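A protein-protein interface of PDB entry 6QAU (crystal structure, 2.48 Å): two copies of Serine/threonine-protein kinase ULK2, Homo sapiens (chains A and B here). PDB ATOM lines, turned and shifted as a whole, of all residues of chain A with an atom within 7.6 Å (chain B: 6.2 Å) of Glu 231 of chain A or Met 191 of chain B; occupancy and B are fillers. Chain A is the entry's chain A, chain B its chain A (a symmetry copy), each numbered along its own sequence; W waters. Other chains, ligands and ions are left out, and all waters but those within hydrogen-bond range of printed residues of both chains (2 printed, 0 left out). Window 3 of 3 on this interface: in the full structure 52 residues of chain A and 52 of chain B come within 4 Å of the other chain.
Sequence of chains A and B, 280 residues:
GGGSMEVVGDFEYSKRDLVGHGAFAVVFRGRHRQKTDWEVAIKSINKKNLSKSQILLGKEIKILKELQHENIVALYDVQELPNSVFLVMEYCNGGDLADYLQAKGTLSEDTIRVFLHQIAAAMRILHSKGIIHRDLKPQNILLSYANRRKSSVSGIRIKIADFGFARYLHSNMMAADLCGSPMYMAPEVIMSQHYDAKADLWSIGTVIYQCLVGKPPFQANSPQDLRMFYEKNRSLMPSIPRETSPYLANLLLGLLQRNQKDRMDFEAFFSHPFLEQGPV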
ATOM      1  N   TYR A 195       8.227  -4.915  16.785  1.00  0.00           N
ATOM      2  CA  TYR A 195       7.435  -5.809  17.586  1.00  0.00           C
ATOM      3  C   TYR A 195       7.284  -5.249  19.018  1.00  0.00           C
ATOM      4  O   TYR A 195       6.325  -5.551  19.698  1.00  0.00           O
ATOM      5  CB  TYR A 195       8.057  -7.207  17.545  1.00  0.00           C
ATOM      6  CG  TYR A 195       7.057  -8.316  17.664  1.00  0.00           C
ATOM      7  CD1 TYR A 195       6.221  -8.653  16.610  1.00  0.00           C
ATOM      8  CD2 TYR A 195       6.877  -8.964  18.869  1.00  0.00           C
ATOM      9  CE1 TYR A 195       5.262  -9.644  16.741  1.00  0.00           C
ATOM     10  CE2 TYR A 195       5.921  -9.955  19.023  1.00  0.00           C
ATOM     11  CZ  TYR A 195       5.112 -10.305  17.956  1.00  0.00           C
ATOM     12  OH  TYR A 195       4.184 -11.302  18.107  1.00  0.00           O
ATOM     13  N   GLN A 224      12.075 -17.971  34.588  1.00  0.00           N
ATOM     14  CA  GLN A 224      11.779 -19.185  33.802  1.00  0.00           C
ATOM     15  C   GLN A 224      10.264 -19.368  33.655  1.00  0.00           C
ATOM     16  O   GLN A 224       9.740 -19.497  32.532  1.00  0.00           O
ATOM     17  CB  GLN A 224      12.365 -20.435  34.472  1.00  0.00           C
ATOM     18  CG  GLN A 224      13.886 -20.438  34.575  1.00  0.00           C
ATOM     19  CD  GLN A 224      14.550 -20.121  33.255  1.00  0.00           C
ATOM     20  OE1 GLN A 224      14.369 -20.826  32.260  1.00  0.00           O
ATOM     21  NE2 GLN A 224      15.326 -19.047  33.234  1.00  0.00           N
ATOM     22  N   ASP A 225       9.581 -19.421  34.807  1.00  0.00           N
ATOM     23  CA  ASP A 225       8.143 -19.681  34.891  1.00  0.00           C
ATOM     24  C   ASP A 225       7.393 -18.634  34.057  1.00  0.00           C
ATOM     25  O   ASP A 225       6.533 -18.980  33.240  1.00  0.00           O
ATOM     26  CB  ASP A 225       7.661 -19.688  36.349  1.00  0.00           C
ATOM     27  CG  ASP A 225       8.288 -20.765  37.226  1.00  0.00           C
ATOM     28  OD1 ASP A 225       8.681 -21.830  36.684  1.00  0.00           O
ATOM     29  OD2 ASP A 225       8.383 -20.528  38.448  1.00  0.00           O
ATOM     30  N   LEU A 226       7.761 -17.359  34.241  1.00  0.00           N
ATOM     31  CA  LEU A 226       7.062 -16.272  33.605  1.00  0.00           C
ATOM     32  C   LEU A 226       7.252 -16.328  32.091  1.00  0.00           C
ATOM     33  O   LEU A 226       6.292 -16.085  31.352  1.00  0.00           O
ATOM     34  CB  LEU A 226       7.526 -14.928  34.166  1.00  0.00           C
ATOM     35  CG  LEU A 226       6.594 -13.768  33.831  1.00  0.00           C
ATOM     36  CD1 LEU A 226       5.278 -13.907  34.583  1.00  0.00           C
ATOM     37  CD2 LEU A 226       7.240 -12.435  34.132  1.00  0.00           C
ATOM     38  N   ARG A 227       8.470 -16.633  31.627  1.00  0.00           N
ATOM     39  CA  ARG A 227       8.694 -16.774  30.184  1.00  0.00           C
ATOM     40  C   ARG A 227       7.701 -17.819  29.638  1.00  0.00           C
ATOM     41  O   ARG A 227       6.891 -17.510  28.759  1.00  0.00           O
ATOM     42  CB  ARG A 227      10.158 -17.124  29.883  1.00  0.00           C
ATOM     43  CG  ARG A 227      10.580 -16.957  28.424  1.00  0.00           C
ATOM     44  CD  ARG A 227      12.047 -17.323  28.203  1.00  0.00           C
ATOM     45  NE  ARG A 227      12.442 -18.559  28.897  1.00  0.00           N
ATOM     46  CZ  ARG A 227      12.539 -19.764  28.332  1.00  0.00           C
ATOM     47  NH1 ARG A 227      12.797 -19.871  27.038  1.00  0.00           N
ATOM     48  NH2 ARG A 227      12.346 -20.850  29.061  1.00  0.00           N
ATOM     49  N   MET A 228       7.727 -19.026  30.217  1.00  0.00           N
ATOM     50  CA  MET A 228       6.979 -20.180  29.682  1.00  0.00           C
ATOM     51  C   MET A 228       5.469 -19.937  29.791  1.00  0.00           C
ATOM     52  O   MET A 228       4.732 -20.208  28.851  1.00  0.00           O
ATOM     53  CB  MET A 228       7.341 -21.475  30.414  1.00  0.00           C
ATOM     54  CG  MET A 228       8.500 -22.226  29.770  1.00  0.00           C
ATOM     55  SD  MET A 228       8.813 -23.829  30.580  1.00  0.00           S
ATOM     56  CE  MET A 228       8.746 -23.386  32.319  1.00  0.00           C
ATOM     57  N   PHE A 229       5.021 -19.410  30.932  1.00  0.00           N
ATOM     58  CA  PHE A 229       3.614 -19.058  31.123  1.00  0.00           C
ATOM     59  C   PHE A 229       3.141 -18.147  29.974  1.00  0.00           C
ATOM     60  O   PHE A 229       2.024 -18.306  29.469  1.00  0.00           O
ATOM     61  CB  PHE A 229       3.425 -18.427  32.501  1.00  0.00           C
ATOM     62  CG  PHE A 229       2.104 -17.745  32.712  1.00  0.00           C
ATOM     63  CD1 PHE A 229       0.967 -18.482  32.984  1.00  0.00           C
ATOM     64  CD2 PHE A 229       1.999 -16.369  32.641  1.00  0.00           C
ATOM     65  CE1 PHE A 229      -0.247 -17.855  33.197  1.00  0.00           C
ATOM     66  CE2 PHE A 229       0.787 -15.739  32.866  1.00  0.00           C
ATOM     67  CZ  PHE A 229      -0.333 -16.480  33.144  1.00  0.00           C
ATOM     68  N   TYR A 230       4.012 -17.221  29.542  1.00  0.00           N
ATOM     69  CA  TYR A 230       3.681 -16.250  28.462  1.00  0.00           C
ATOM     70  C   TYR A 230       3.798 -16.934  27.089  1.00  0.00           C
ATOM     71  O   TYR A 230       3.084 -16.568  26.161  1.00  0.00           O
ATOM     72  CB  TYR A 230       4.587 -15.009  28.495  1.00  0.00           C
ATOM     73  CG  TYR A 230       4.303 -13.966  29.550  1.00  0.00           C
ATOM     74  CD1 TYR A 230       3.034 -13.772  30.070  1.00  0.00           C
ATOM     75  CD2 TYR A 230       5.315 -13.127  30.002  1.00  0.00           C
ATOM     76  CE1 TYR A 230       2.784 -12.805  31.038  1.00  0.00           C
ATOM     77  CE2 TYR A 230       5.079 -12.133  30.946  1.00  0.00           C
ATOM     78  CZ  TYR A 230       3.803 -11.973  31.468  1.00  0.00           C
ATOM     79  OH  TYR A 230       3.543 -11.032  32.420  1.00  0.00           O
ATOM     80  N   GLU A 231       4.740 -17.885  26.971  1.00  0.00           N
ATOM     81  CA  GLU A 231       4.952 -18.728  25.778  1.00  0.00           C
ATOM     82  C   GLU A 231       3.689 -19.548  25.495  1.00  0.00           C
ATOM     83  O   GLU A 231       3.221 -19.584  24.368  1.00  0.00           O
ATOM     84  CB  GLU A 231       6.118 -19.685  26.040  1.00  0.00           C
ATOM     85  CG  GLU A 231       7.229 -19.677  25.004  1.00  0.00           C
ATOM     86  CD  GLU A 231       8.542 -20.255  25.537  1.00  0.00           C
ATOM     87  OE1 GLU A 231       9.135 -19.624  26.447  1.00  0.00           O
ATOM     88  OE2 GLU A 231       8.959 -21.355  25.071  1.00  0.00           O
ATOM     89  N   LYS A 232       3.156 -20.189  26.552  1.00  0.00           N
ATOM     90  CA  LYS A 232       2.105 -21.224  26.442  1.00  0.00           C
ATOM     91  C   LYS A 232       0.750 -20.552  26.257  1.00  0.00           C
ATOM     92  O   LYS A 232      -0.009 -20.926  25.385  1.00  0.00           O
ATOM     93  CB  LYS A 232       2.063 -22.130  27.681  1.00  0.00           C
ATOM     94  CG  LYS A 232       3.031 -23.306  27.658  1.00  0.00           C
ATOM     95  CD  LYS A 232       2.617 -24.448  28.546  1.00  0.00           C
ATOM     96  CE  LYS A 232       3.652 -25.547  28.588  1.00  0.00           C
ATOM     97  NZ  LYS A 232       3.301 -26.550  29.611  1.00  0.00           N
ATOM     98  N   ASN A 233       0.458 -19.582  27.123  1.00  0.00           N
ATOM     99  CA  ASN A 233      -0.806 -18.878  27.102  1.00  0.00           C
ATOM    100  C   ASN A 233      -0.682 -17.689  26.138  1.00  0.00           C
ATOM    101  O   ASN A 233      -0.121 -16.658  26.502  1.00  0.00           O
ATOM    102  CB  ASN A 233      -1.221 -18.444  28.513  1.00  0.00           C
ATOM    103  CG  ASN A 233      -1.251 -19.579  29.518  1.00  0.00           C
ATOM    104  OD1 ASN A 233      -2.245 -20.299  29.625  1.00  0.00           O
ATOM    105  ND2 ASN A 233      -0.176 -19.727  30.284  1.00  0.00           N
ATOM    106  N   ARG A 234      -1.204 -17.840  24.910  1.00  0.00           N
ATOM    107  CA  ARG A 234      -1.092 -16.811  23.846  1.00  0.00           C
ATOM    108  C   ARG A 234      -2.178 -15.740  24.034  1.00  0.00           C
ATOM    109  O   ARG A 234      -2.175 -14.734  23.320  1.00  0.00           O
ATOM    110  CB  ARG A 234      -1.207 -17.433  22.446  1.00  0.00           C
ATOM    111  CG  ARG A 234       0.072 -18.065  21.901  1.00  0.00           C
ATOM    112  CD  ARG A 234      -0.138 -18.688  20.530  1.00  0.00           C
ATOM    113  NE  ARG A 234       0.640 -19.912  20.328  1.00  0.00           N
ATOM    114  CZ  ARG A 234       0.240 -20.962  19.599  1.00  0.00           C
ATOM    115  NH1 ARG A 234      -0.954 -20.968  19.025  1.00  0.00           N
ATOM    116  NH2 ARG A 234       1.033 -22.009  19.449  1.00  0.00           N
ATOM    117  N   SER A 235      -3.096 -15.967  24.995  1.00  0.00           N
ATOM    118  CA  SER A 235      -4.165 -15.018  25.378  1.00  0.00           C
ATOM    119  C   SER A 235      -4.402 -15.057  26.899  1.00  0.00           C
ATOM    120  O   SER A 235      -4.718 -16.108  27.434  1.00  0.00           O
ATOM    121  CB  SER A 235      -5.433 -15.346  24.630  1.00  0.00           C
ATOM    122  OG  SER A 235      -6.480 -14.452  24.979  1.00  0.00           O
ATOM    123  N   LEU A 236      -4.271 -13.904  27.575  1.00  0.00           N
ATOM    124  CA  LEU A 236      -4.412 -13.814  29.046  1.00  0.00           C
ATOM    125  C   LEU A 236      -5.447 -12.751  29.437  1.00  0.00           C
ATOM    126  O   LEU A 236      -5.443 -11.676  28.870  1.00  0.00           O
ATOM    127  CB  LEU A 236      -3.039 -13.477  29.643  1.00  0.00           C
ATOM    128  CG  LEU A 236      -2.035 -14.622  29.597  1.00  0.00           C
ATOM    129  CD1 LEU A 236      -0.711 -14.203  30.204  1.00  0.00           C
ATOM    130  CD2 LEU A 236      -2.599 -15.853  30.304  1.00  0.00           C
ATOM    131  N   ARG A 258      -1.626  -9.507  26.067  1.00  0.00           N
ATOM    132  CA  ARG A 258      -0.484 -10.379  25.899  1.00  0.00           C
ATOM    133  C   ARG A 258       0.091 -10.214  24.493  1.00  0.00           C
ATOM    134  O   ARG A 258       1.282 -10.210  24.316  1.00  0.00           O
ATOM    135  CB  ARG A 258      -0.880 -11.833  26.147  1.00  0.00           C
ATOM    136  CG  ARG A 258       0.312 -12.765  26.267  1.00  0.00           C
ATOM    137  CD  ARG A 258       0.976 -13.063  24.947  1.00  0.00           C
ATOM    138  NE  ARG A 258       1.721 -14.302  24.962  1.00  0.00           N
ATOM    139  CZ  ARG A 258       2.754 -14.537  24.181  1.00  0.00           C
ATOM    140  NH1 ARG A 258       3.480 -13.521  23.725  1.00  0.00           N
ATOM    141  NH2 ARG A 258       3.045 -15.783  23.835  1.00  0.00           N
ATOM    142  N   HIS B 170      18.644  -9.136  21.714  1.00  0.00           N
ATOM    143  CA  HIS B 170      18.835  -9.907  22.947  1.00  0.00           C
ATOM    144  C   HIS B 170      18.304 -11.356  22.792  1.00  0.00           C
ATOM    145  O   HIS B 170      17.392 -11.638  22.004  1.00  0.00           O
ATOM    146  CB  HIS B 170      18.234  -9.143  24.135  1.00  0.00           C
ATOM    147  CG  HIS B 170      16.741  -9.071  24.158  1.00  0.00           C
ATOM    148  ND1 HIS B 170      16.029  -8.236  23.330  1.00  0.00           N
ATOM    149  CD2 HIS B 170      15.828  -9.699  24.936  1.00  0.00           C
ATOM    150  CE1 HIS B 170      14.738  -8.374  23.577  1.00  0.00           C
ATOM    151  NE2 HIS B 170      14.592  -9.264  24.557  1.00  0.00           N
ATOM    152  N   ASN B 172      17.029 -14.859  25.474  1.00  0.00           N
ATOM    153  CA  ASN B 172      15.949 -14.986  26.488  1.00  0.00           C
ATOM    154  C   ASN B 172      16.408 -14.426  27.844  1.00  0.00           C
ATOM    155  O   ASN B 172      15.721 -13.586  28.430  1.00  0.00           O
ATOM    156  CB  ASN B 172      15.457 -16.429  26.638  1.00  0.00           C
ATOM    157  CG  ASN B 172      14.320 -16.769  25.697  1.00  0.00           C
ATOM    158  OD1 ASN B 172      13.480 -15.920  25.399  1.00  0.00           O
ATOM    159  ND2 ASN B 172      14.278 -18.008  25.232  1.00  0.00           N
ATOM    160  N   ALA B 186       7.435  -6.534  29.180  1.00  0.00           N
ATOM    161  CA  ALA B 186       6.516  -6.914  28.126  1.00  0.00           C
ATOM    162  C   ALA B 186       6.802  -8.334  27.674  1.00  0.00           C
ATOM    163  O   ALA B 186       7.950  -8.727  27.556  1.00  0.00           O
ATOM    164  CB  ALA B 186       6.638  -5.970  26.966  1.00  0.00           C
ATOM    165  N   PRO B 187       5.762  -9.142  27.363  1.00  0.00           N
ATOM    166  CA  PRO B 187       5.968 -10.512  26.890  1.00  0.00           C
ATOM    167  C   PRO B 187       6.857 -10.602  25.649  1.00  0.00           C
ATOM    168  O   PRO B 187       7.663 -11.513  25.551  1.00  0.00           O
ATOM    169  CB  PRO B 187       4.546 -10.997  26.596  1.00  0.00           C
ATOM    170  CG  PRO B 187       3.721 -10.198  27.575  1.00  0.00           C
ATOM    171  CD  PRO B 187       4.339  -8.820  27.534  1.00  0.00           C
ATOM    172  N   GLU B 188       6.710  -9.653  24.732  1.00  0.00           N
ATOM    173  CA  GLU B 188       7.483  -9.702  23.507  1.00  0.00           C
ATOM    174  C   GLU B 188       8.976  -9.405  23.817  1.00  0.00           C
ATOM    175  O   GLU B 188       9.841  -9.860  23.124  1.00  0.00           O
ATOM    176  CB  GLU B 188       6.885  -8.769  22.452  1.00  0.00           C
ATOM    177  CG  GLU B 188       6.947  -7.292  22.801  1.00  0.00           C
ATOM    178  CD  GLU B 188       5.730  -6.723  23.505  1.00  0.00           C
ATOM    179  OE1 GLU B 188       4.970  -7.531  24.068  1.00  0.00           O
ATOM    180  OE2 GLU B 188       5.535  -5.453  23.423  1.00  0.00           O
ATOM    181  N   VAL B 189       9.269  -8.665  24.883  1.00  0.00           N
ATOM    182  CA  VAL B 189      10.637  -8.438  25.293  1.00  0.00           C
ATOM    183  C   VAL B 189      11.203  -9.691  26.007  1.00  0.00           C
ATOM    184  O   VAL B 189      12.321 -10.090  25.749  1.00  0.00           O
ATOM    185  CB  VAL B 189      10.752  -7.177  26.162  1.00  0.00           C
ATOM    186  CG1 VAL B 189      12.144  -7.018  26.759  1.00  0.00           C
ATOM    187  CG2 VAL B 189      10.381  -5.936  25.382  1.00  0.00           C
ATOM    188  N   ILE B 190      10.426 -10.307  26.900  1.00  0.00           N
ATOM    189  CA  ILE B 190      10.835 -11.508  27.613  1.00  0.00           C
ATOM    190  C   ILE B 190      11.122 -12.636  26.609  1.00  0.00           C
ATOM    191  O   ILE B 190      11.998 -13.444  26.816  1.00  0.00           O
ATOM    192  CB  ILE B 190       9.762 -11.929  28.625  1.00  0.00           C
ATOM    193  CG1 ILE B 190       9.666 -10.938  29.779  1.00  0.00           C
ATOM    194  CG2 ILE B 190       9.997 -13.337  29.142  1.00  0.00           C
ATOM    195  CD1 ILE B 190       8.546 -11.249  30.739  1.00  0.00           C
ATOM    196  N   MET B 191      10.347 -12.697  25.526  1.00  0.00           N
ATOM    197  CA  MET B 191      10.373 -13.817  24.607  1.00  0.00           C
ATOM    198  C   MET B 191      11.294 -13.536  23.416  1.00  0.00           C
ATOM    199  O   MET B 191      11.495 -14.381  22.570  1.00  0.00           O
ATOM    200  CB  MET B 191       8.947 -14.137  24.126  1.00  0.00           C
ATOM    201  CG  MET B 191       8.125 -14.857  25.201  1.00  0.00           C
ATOM    202  SD  MET B 191       6.367 -15.109  24.792  1.00  0.00           S
ATOM    203  CE  MET B 191       6.487 -15.961  23.218  1.00  0.00           C
ATOM    204  N   SER B 192      11.818 -12.327  23.306  1.00  0.00           N
ATOM    205  CA  SER B 192      12.808 -11.972  22.267  1.00  0.00           C
ATOM    206  C   SER B 192      12.185 -12.025  20.875  1.00  0.00           C
ATOM    207  O   SER B 192      12.769 -12.535  19.945  1.00  0.00           O
ATOM    208  CB  SER B 192      14.033 -12.835  22.322  1.00  0.00           C
ATOM    209  OG  SER B 192      14.769 -12.590  23.513  1.00  0.00           O
ATOM    210  N   GLN B 193      10.999 -11.455  20.748  1.00  0.00           N
ATOM    211  CA  GLN B 193      10.306 -11.445  19.481  1.00  0.00           C
ATOM    212  C   GLN B 193      10.696 -10.160  18.760  1.00  0.00           C
ATOM    213  O   GLN B 193      10.619  -9.071  19.335  1.00  0.00           O
ATOM    214  CB  GLN B 193       8.795 -11.596  19.683  1.00  0.00           C
ATOM    215  CG  GLN B 193       8.392 -12.981  20.166  1.00  0.00           C
ATOM    216  CD  GLN B 193       6.938 -13.092  20.532  1.00  0.00           C
ATOM    217  OE1 GLN B 193       6.344 -12.173  21.096  1.00  0.00           O
ATOM    218  NE2 GLN B 193       6.377 -14.263  20.265  1.00  0.00           N
HETATM  219  O   HOH W   1       4.117 -15.780  20.924  1.00  0.00           O
HETATM  220  O   HOH W   2       3.421  -9.743  22.181  1.00  0.00           O
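Water W1 lies within hydrogen-bond range of the side-chain amide nitrogen of Gln 193 of chain B (2.8 Å) and the guanidinium group of Arg 258 of chain A (3.1 Å). Water W2 lies within hydrogen-bond range of the backbone carbonyl oxygen of Arg 258 of chain A (3.1 Å) and the side-chain carboxylate of Glu 188 of chain B (3.3 Å).
Hydrophobic or aromatic side chains of chain B within 4 Å of the printed part of chain A: Pro 187, Ile 190 and Met 191. Of the 15 printed residues of chain A, 6 touch a printed residue of chain B. Printed residues of chain A that touch a printed residue of chain B: Tyr 195, Leu 226, Arg 227, Tyr 230, Glu 231 and Arg 258. Along chain A the printed residues that touch a printed residue of chain B span positions 195 to 258.
Of chain A, only Tyr 230, Glu 231 and Arg 258 come within 4 Å of Met 191 of chain B. Of the printed residues of chain B, Arg 227 of chain A touches Asn 172 (3.0 Å) and Ile 190 (3.7 Å). Of the printed residues of chain B, Tyr 195 of chain A touches Glu 188 (3.6 Å) and Gln 193 (3.1 Å). Lys 232 of chain A touches none of the printed residues of chain B.
Glu 188 of chain B touches Tyr 195 of chain A. Gln 193 of chain B touches Tyr 195 of chain A. CD2 of Leu 226 of chain A touches CD1 of Ile 190 of chain B, 3.8 Å away. Arg 227 of chain A touches Ile 190 of chain B (CG to CG2, 3.7 Å). Ile 190 of chain B touches Tyr 230 of chain A (CD1 to CE2, 3.6 Å). Tyr 230 of chain A touches Met 191 of chain B (O to SD, 3.8 Å). Met 191 of chain B touches Glu 231 of chain A (SD to N, 3.9 Å). Arg 258 of chain A touches Pro 187 of chain B.
OE1 of Glu 231 of chain A is in salt-bridge range of NH1 of Arg 227 of chain A, at 3.7 Å. The backbone carbonyl oxygen (O) of Tyr 230 of chain A is in hydrogen-bond range of the guanidinium group (NH2) of Arg 258 of chain A (2.5 Å). NE of Arg 258 of chain A lies within hydrogen-bond range of O of Asn 233 of chain A, at 3.4 Å. OD1 of Asn 172 of chain B lies close to O of Ile 190 of chain B (3.2 Å). The backbone NH of Gln 193 of chain B lies within hydrogen-bond range of the backbone carbonyl oxygen of Glu 188 of chain B (3.1 Å).
No position is printed for both chains. Of the 10 pairs that touch across the chains among the printed residues, none has its exchanged pair printed and touching as well.
NH1 of Arg 227 of chain A sits close to ND2 of Asn 172 of chain B (3.0 Å). The side-chain sulfur of Met 191 of chain B sits at hydrogen-bond distance from the guanidinium group of Arg 258 of chain A.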
